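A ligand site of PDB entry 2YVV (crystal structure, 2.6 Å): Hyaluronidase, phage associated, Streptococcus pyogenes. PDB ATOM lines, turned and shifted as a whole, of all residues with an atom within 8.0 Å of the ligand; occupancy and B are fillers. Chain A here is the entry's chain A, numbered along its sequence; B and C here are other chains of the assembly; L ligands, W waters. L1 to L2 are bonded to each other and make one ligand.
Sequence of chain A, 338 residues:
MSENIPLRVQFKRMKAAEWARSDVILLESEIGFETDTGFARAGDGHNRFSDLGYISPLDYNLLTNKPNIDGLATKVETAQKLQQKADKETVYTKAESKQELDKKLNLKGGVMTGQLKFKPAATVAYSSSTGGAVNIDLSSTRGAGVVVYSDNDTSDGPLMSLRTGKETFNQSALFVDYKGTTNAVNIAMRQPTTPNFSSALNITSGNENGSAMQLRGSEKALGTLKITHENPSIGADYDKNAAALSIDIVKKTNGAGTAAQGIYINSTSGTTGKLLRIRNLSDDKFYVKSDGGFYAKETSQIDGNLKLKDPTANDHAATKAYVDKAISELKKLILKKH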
ATOM      1  N   ARG A 163     -21.441  -1.417 -20.127  1.00  0.00           N
ATOM      2  CA  ARG A 163     -21.117  -1.365 -18.688  1.00  0.00           C
ATOM      3  C   ARG A 163     -22.245  -0.709 -17.874  1.00  0.00           C
ATOM      4  O   ARG A 163     -22.779   0.340 -18.248  1.00  0.00           O
ATOM      5  CB  ARG A 163     -19.786  -0.626 -18.456  1.00  0.00           C
ATOM      6  CG  ARG A 163     -19.154  -0.776 -17.019  1.00  0.00           C
ATOM      7  CD  ARG A 163     -17.995   0.224 -16.711  1.00  0.00           C
ATOM      8  NE  ARG A 163     -18.394   1.617 -17.026  1.00  0.00           N
ATOM      9  CZ  ARG A 163     -19.052   2.438 -16.201  1.00  0.00           C
ATOM     10  NH1 ARG A 163     -19.401   2.017 -14.987  1.00  0.00           N
ATOM     11  NH2 ARG A 163     -19.390   3.667 -16.569  1.00  0.00           N
ATOM     12  N   THR A 164     -22.616  -1.348 -16.777  1.00  0.00           N
ATOM     13  CA  THR A 164     -23.491  -0.685 -15.822  1.00  0.00           C
ATOM     14  C   THR A 164     -22.820  -0.604 -14.450  1.00  0.00           C
ATOM     15  O   THR A 164     -22.255  -1.593 -13.953  1.00  0.00           O
ATOM     16  CB  THR A 164     -24.814  -1.399 -15.694  1.00  0.00           C
ATOM     17  OG1 THR A 164     -24.575  -2.783 -15.368  1.00  0.00           O
ATOM     18  CG2 THR A 164     -25.571  -1.247 -17.003  1.00  0.00           C
ATOM     19  N   GLY A 165     -22.871   0.572 -13.832  1.00  0.00           N
ATOM     20  CA  GLY A 165     -22.078   0.828 -12.636  1.00  0.00           C
ATOM     21  C   GLY A 165     -22.793   0.676 -11.285  1.00  0.00           C
ATOM     22  O   GLY A 165     -22.138   0.615 -10.268  1.00  0.00           O
ATOM     23  N   LYS A 166     -24.110   0.591 -11.256  1.00  0.00           N
ATOM     24  CA  LYS A 166     -24.809   0.584  -9.944  1.00  0.00           C
ATOM     25  C   LYS A 166     -25.571  -0.693  -9.683  1.00  0.00           C
ATOM     26  O   LYS A 166     -26.322  -1.148 -10.513  1.00  0.00           O
ATOM     27  CB  LYS A 166     -25.795   1.765  -9.829  1.00  0.00           C
ATOM     28  CG  LYS A 166     -25.192   3.154  -9.901  1.00  0.00           C
ATOM     29  CD  LYS A 166     -24.975   3.747  -8.518  1.00  0.00           C
ATOM     30  CE  LYS A 166     -23.504   3.837  -8.149  1.00  0.00           C
ATOM     31  NZ  LYS A 166     -22.714   5.015  -8.603  1.00  0.00           N
ATOM     32  N   GLU A 167     -25.453  -1.213  -8.473  1.00  0.00           N
ATOM     33  CA  GLU A 167     -26.083  -2.477  -8.142  1.00  0.00           C
ATOM     34  C   GLU A 167     -27.598  -2.536  -8.167  1.00  0.00           C
ATOM     35  O   GLU A 167     -28.198  -3.613  -8.176  1.00  0.00           O
ATOM     36  CB  GLU A 167     -25.507  -2.990  -6.834  1.00  0.00           C
ATOM     37  CG  GLU A 167     -24.410  -4.061  -7.097  1.00  0.00           C
ATOM     38  CD  GLU A 167     -24.972  -5.306  -7.872  1.00  0.00           C
ATOM     39  OE1 GLU A 167     -25.956  -5.916  -7.384  1.00  0.00           O
ATOM     40  OE2 GLU A 167     -24.433  -5.659  -8.961  1.00  0.00           O
ATOM     41  N   TYR B 149     -22.618   2.966 -21.579  1.00  0.00           N
ATOM     42  CA  TYR B 149     -22.612   2.625 -20.172  1.00  0.00           C
ATOM     43  C   TYR B 149     -23.539   3.498 -19.422  1.00  0.00           C
ATOM     44  O   TYR B 149     -23.953   4.571 -19.890  1.00  0.00           O
ATOM     45  CB  TYR B 149     -21.217   2.794 -19.583  1.00  0.00           C
ATOM     46  CG  TYR B 149     -20.696   4.159 -19.883  1.00  0.00           C
ATOM     47  CD1 TYR B 149     -20.203   4.465 -21.161  1.00  0.00           C
ATOM     48  CD2 TYR B 149     -20.756   5.179 -18.929  1.00  0.00           C
ATOM     49  CE1 TYR B 149     -19.750   5.751 -21.473  1.00  0.00           C
ATOM     50  CE2 TYR B 149     -20.290   6.472 -19.224  1.00  0.00           C
ATOM     51  CZ  TYR B 149     -19.789   6.745 -20.501  1.00  0.00           C
ATOM     52  OH  TYR B 149     -19.341   8.002 -20.833  1.00  0.00           O
ATOM     53  N   SER B 150     -23.860   3.071 -18.222  1.00  0.00           N
ATOM     54  CA  SER B 150     -24.680   3.879 -17.387  1.00  0.00           C
ATOM     55  C   SER B 150     -24.244   3.697 -15.960  1.00  0.00           C
ATOM     56  O   SER B 150     -23.961   2.561 -15.522  1.00  0.00           O
ATOM     57  CB  SER B 150     -26.125   3.453 -17.518  1.00  0.00           C
ATOM     58  OG  SER B 150     -26.905   4.127 -16.528  1.00  0.00           O
ATOM     59  N   ASP B 151     -24.165   4.822 -15.245  1.00  0.00           N
ATOM     60  CA  ASP B 151     -23.988   4.793 -13.804  1.00  0.00           C
ATOM     61  C   ASP B 151     -25.229   5.274 -13.055  1.00  0.00           C
ATOM     62  O   ASP B 151     -25.158   5.706 -11.921  1.00  0.00           O
ATOM     63  CB  ASP B 151     -22.737   5.559 -13.429  1.00  0.00           C
ATOM     64  CG  ASP B 151     -21.491   4.821 -13.903  1.00  0.00           C
ATOM     65  OD1 ASP B 151     -21.219   3.722 -13.347  1.00  0.00           O
ATOM     66  OD2 ASP B 151     -20.811   5.301 -14.867  1.00  0.00           O
ATOM     67  N   ASN B 152     -26.385   5.161 -13.704  1.00  0.00           N
ATOM     68  CA  ASN B 152     -27.653   5.564 -13.126  1.00  0.00           C
ATOM     69  C   ASN B 152     -28.170   4.486 -12.190  1.00  0.00           C
ATOM     70  O   ASN B 152     -27.789   3.322 -12.301  1.00  0.00           O
ATOM     71  CB  ASN B 152     -28.647   5.827 -14.224  1.00  0.00           C
ATOM     72  CG  ASN B 152     -29.678   6.863 -13.826  1.00  0.00           C
ATOM     73  OD1 ASN B 152     -29.707   7.284 -12.672  1.00  0.00           O
ATOM     74  ND2 ASN B 152     -30.529   7.278 -14.779  1.00  0.00           N
ATOM     75  N   ASP B 153     -29.011   4.851 -11.253  1.00  0.00           N
ATOM     76  CA  ASP B 153     -29.389   3.882 -10.252  1.00  0.00           C
ATOM     77  C   ASP B 153     -30.389   2.920 -10.830  1.00  0.00           C
ATOM     78  O   ASP B 153     -30.385   1.741 -10.492  1.00  0.00           O
ATOM     79  CB  ASP B 153     -30.019   4.572  -9.054  1.00  0.00           C
ATOM     80  CG  ASP B 153     -29.147   5.660  -8.517  1.00  0.00           C
ATOM     81  OD1 ASP B 153     -28.058   5.328  -7.962  1.00  0.00           O
ATOM     82  OD2 ASP B 153     -29.533   6.842  -8.684  1.00  0.00           O
ATOM     83  N   ARG B 190     -20.304  -9.079 -12.024  1.00  0.00           N
ATOM     84  CA  ARG B 190     -19.513  -8.710 -10.840  1.00  0.00           C
ATOM     85  C   ARG B 190     -20.180  -9.084  -9.529  1.00  0.00           C
ATOM     86  O   ARG B 190     -21.368  -8.884  -9.373  1.00  0.00           O
ATOM     87  CB  ARG B 190     -19.317  -7.172 -10.862  1.00  0.00           C
ATOM     88  CG  ARG B 190     -18.773  -6.609 -12.219  1.00  0.00           C
ATOM     89  CD  ARG B 190     -17.270  -6.882 -12.244  1.00  0.00           C
ATOM     90  NE  ARG B 190     -16.595  -6.505 -13.493  1.00  0.00           N
ATOM     91  CZ  ARG B 190     -15.585  -7.205 -14.020  1.00  0.00           C
ATOM     92  NH1 ARG B 190     -15.179  -8.323 -13.424  1.00  0.00           N
ATOM     93  NH2 ARG B 190     -15.004  -6.807 -15.142  1.00  0.00           N
ATOM     94  N   SER C 129     -14.810   3.986 -19.633  1.00  0.00           N
ATOM     95  CA  SER C 129     -16.064   4.742 -19.840  1.00  0.00           C
ATOM     96  C   SER C 129     -15.867   6.175 -20.419  1.00  0.00           C
ATOM     97  O   SER C 129     -16.635   7.096 -20.106  1.00  0.00           O
ATOM     98  CB  SER C 129     -16.902   4.785 -18.547  1.00  0.00           C
ATOM     99  OG  SER C 129     -16.304   5.567 -17.528  1.00  0.00           O
ATOM    100  N   THR C 130     -14.853   6.338 -21.268  1.00  0.00           N
ATOM    101  CA  THR C 130     -14.596   7.632 -21.921  1.00  0.00           C
ATOM    102  C   THR C 130     -13.921   7.457 -23.310  1.00  0.00           C
ATOM    103  O   THR C 130     -13.516   8.446 -23.964  1.00  0.00           O
ATOM    104  CB  THR C 130     -13.837   8.634 -20.962  1.00  0.00           C
ATOM    105  OG1 THR C 130     -13.529   9.859 -21.650  1.00  0.00           O
ATOM    106  CG2 THR C 130     -12.558   8.024 -20.415  1.00  0.00           C
ATOM    107  N   ASP C 137     -23.399   7.759 -22.791  1.00  0.00           N
ATOM    108  CA  ASP C 137     -23.417   7.813 -21.340  1.00  0.00           C
ATOM    109  C   ASP C 137     -24.864   8.042 -20.937  1.00  0.00           C
ATOM    110  O   ASP C 137     -25.404   9.143 -21.156  1.00  0.00           O
ATOM    111  CB  ASP C 137     -22.556   8.978 -20.854  1.00  0.00           C
ATOM    112  CG  ASP C 137     -22.566   9.147 -19.331  1.00  0.00           C
ATOM    113  OD1 ASP C 137     -23.314   8.444 -18.605  1.00  0.00           O
ATOM    114  OD2 ASP C 137     -21.800   9.992 -18.844  1.00  0.00           O
ATOM    115  N   SER C 139     -25.930   7.757 -17.790  1.00  0.00           N
ATOM    116  CA  SER C 139     -25.924   8.012 -16.347  1.00  0.00           C
ATOM    117  C   SER C 139     -26.982   8.962 -15.792  1.00  0.00           C
ATOM    118  O   SER C 139     -27.346   8.840 -14.640  1.00  0.00           O
ATOM    119  CB  SER C 139     -24.542   8.452 -15.864  1.00  0.00           C
ATOM    120  OG  SER C 139     -23.588   7.462 -16.179  1.00  0.00           O
ATOM    121  N   ASP C 177     -19.878  -5.792 -18.903  1.00  0.00           N
ATOM    122  CA  ASP C 177     -19.451  -5.624 -17.516  1.00  0.00           C
ATOM    123  C   ASP C 177     -20.692  -5.151 -16.763  1.00  0.00           C
ATOM    124  O   ASP C 177     -21.103  -3.990 -16.875  1.00  0.00           O
ATOM    125  CB  ASP C 177     -18.344  -4.570 -17.482  1.00  0.00           C
ATOM    126  CG  ASP C 177     -17.721  -4.361 -16.088  1.00  0.00           C
ATOM    127  OD1 ASP C 177     -18.158  -5.003 -15.110  1.00  0.00           O
ATOM    128  OD2 ASP C 177     -16.763  -3.543 -15.980  1.00  0.00           O
ATOM    129  N   TYR C 178     -21.330  -6.032 -16.017  1.00  0.00           N
ATOM    130  CA  TYR C 178     -22.684  -5.705 -15.580  1.00  0.00           C
ATOM    131  C   TYR C 178     -22.832  -5.697 -14.090  1.00  0.00           C
ATOM    132  O   TYR C 178     -22.435  -6.643 -13.441  1.00  0.00           O
ATOM    133  CB  TYR C 178     -23.679  -6.717 -16.094  1.00  0.00           C
ATOM    134  CG  TYR C 178     -25.090  -6.451 -15.678  1.00  0.00           C
ATOM    135  CD1 TYR C 178     -25.874  -5.505 -16.351  1.00  0.00           C
ATOM    136  CD2 TYR C 178     -25.676  -7.176 -14.621  1.00  0.00           C
ATOM    137  CE1 TYR C 178     -27.215  -5.282 -15.984  1.00  0.00           C
ATOM    138  CE2 TYR C 178     -27.026  -6.961 -14.249  1.00  0.00           C
ATOM    139  CZ  TYR C 178     -27.793  -6.015 -14.947  1.00  0.00           C
ATOM    140  OH  TYR C 178     -29.128  -5.776 -14.620  1.00  0.00           O
ATOM    141  N   LYS C 179     -23.463  -4.646 -13.579  1.00  0.00           N
ATOM    142  CA  LYS C 179     -23.977  -4.616 -12.191  1.00  0.00           C
ATOM    143  C   LYS C 179     -25.441  -4.296 -12.288  1.00  0.00           C
ATOM    144  O   LYS C 179     -25.796  -3.467 -13.093  1.00  0.00           O
ATOM    145  CB  LYS C 179     -23.268  -3.560 -11.343  1.00  0.00           C
ATOM    146  CG  LYS C 179     -21.842  -3.937 -11.119  1.00  0.00           C
ATOM    147  CD  LYS C 179     -21.171  -3.188  -9.991  1.00  0.00           C
ATOM    148  CE  LYS C 179     -19.634  -3.286 -10.167  1.00  0.00           C
ATOM    149  NZ  LYS C 179     -18.919  -2.651  -9.023  1.00  0.00           N
HETATM  150  C1  LIG L   1     -17.550   1.559 -10.078  1.00  0.00           C
HETATM  151  C2  LIG L   1     -19.021   1.589  -9.744  1.00  0.00           C
HETATM  152  C3  LIG L   1     -19.608   3.014 -10.204  1.00  0.00           C
HETATM  153  C4  LIG L   1     -18.881   4.092  -9.378  1.00  0.00           C
HETATM  154  C5  LIG L   1     -17.333   3.990  -9.620  1.00  0.00           C
HETATM  155  C6  LIG L   1     -16.561   5.033  -8.745  1.00  0.00           C
HETATM  156  O1  LIG L   1     -17.460   1.755 -11.519  1.00  0.00           O
HETATM  157  O2  LIG L   1     -19.642   0.511 -10.455  1.00  0.00           O
HETATM  158  O3  LIG L   1     -21.021   3.107  -9.925  1.00  0.00           O
HETATM  159  O4  LIG L   1     -19.174   5.552  -9.465  1.00  0.00           O
HETATM  160  O5  LIG L   1     -16.845   2.614  -9.338  1.00  0.00           O
HETATM  161  O6  LIG L   1     -15.152   4.904  -8.954  1.00  0.00           O
HETATM  162  C1  LG2 L   2     -19.811   6.360 -10.553  1.00  0.00           C
HETATM  163  C2  LG2 L   2     -19.889   7.749  -9.808  1.00  0.00           C
HETATM  164  C3  LG2 L   2     -20.474   8.850 -10.673  1.00  0.00           C
HETATM  165  C4  LG2 L   2     -19.545   8.906 -11.955  1.00  0.00           C
HETATM  166  C5  LG2 L   2     -19.460   7.533 -12.740  1.00  0.00           C
HETATM  167  C6  LG2 L   2     -18.439   7.736 -13.943  1.00  0.00           C
HETATM  168  O1  LG2 L   2     -20.707   7.625  -8.636  1.00  0.00           O
HETATM  169  O2  LG2 L   2     -20.483  10.139  -9.878  1.00  0.00           O
HETATM  170  O3  LG2 L   2     -18.217   9.383 -11.597  1.00  0.00           O
HETATM  171  O4  LG2 L   2     -18.918   6.564 -11.736  1.00  0.00           O
HETATM  172  O5  LG2 L   2     -19.007   7.597 -15.265  1.00  0.00           O
HETATM  173  O   HOH W   1     -16.047   0.017 -12.755  1.00  0.00           O
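NH1 of Arg 163 touches O1 of LIG L1, at 3.98 Å.
Lys 179 of chain C touches the ligand.
Five residues have an atom within 4 Å of the ligand: Arg 163, Gly 165, Lys 166, Asp 151 of chain B and Lys 179 of chain C.
The nearest printed residue that does not touch the ligand is Ser 129 of chain C (4.1 Å).
The backbone carbonyl oxygen (O) of Gly 165 lies within hydrogen-bond range of an oxygen (O2) of LIG L1 (2.5 Å).
The side-chain carboxylate (OD2) of Asp 151 of chain B is in hydrogen-bond range of an oxygen (O5) of LG2 L2, 2.9 Å away.
The side-chain amino group (NZ) of Lys 166 is in hydrogen-bond range of an oxygen (O3) of LIG L1 (2.9 Å).
The backbone carbonyl oxygen (O) of Lys 179 of chain C lies within hydrogen-bond range of the side-chain hydroxyl (OG1) of Thr 164, 2.7 Å away.
O of Arg 163 sits at hydrogen-bond distance from N of Ser 150 of chain B, at 2.9 Å.
NH2 of Arg 163 is in salt-bridge range of OD2 of Asp 151 of chain B (2.8 Å).
The backbone NH of Gly 165 sits at hydrogen-bond distance from the backbone carbonyl oxygen of Ser 150 of chain B, at 2.8 Å.
N of Asp 151 of chain B sits at hydrogen-bond distance from OG of Ser 139 of chain C (2.9 Å).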
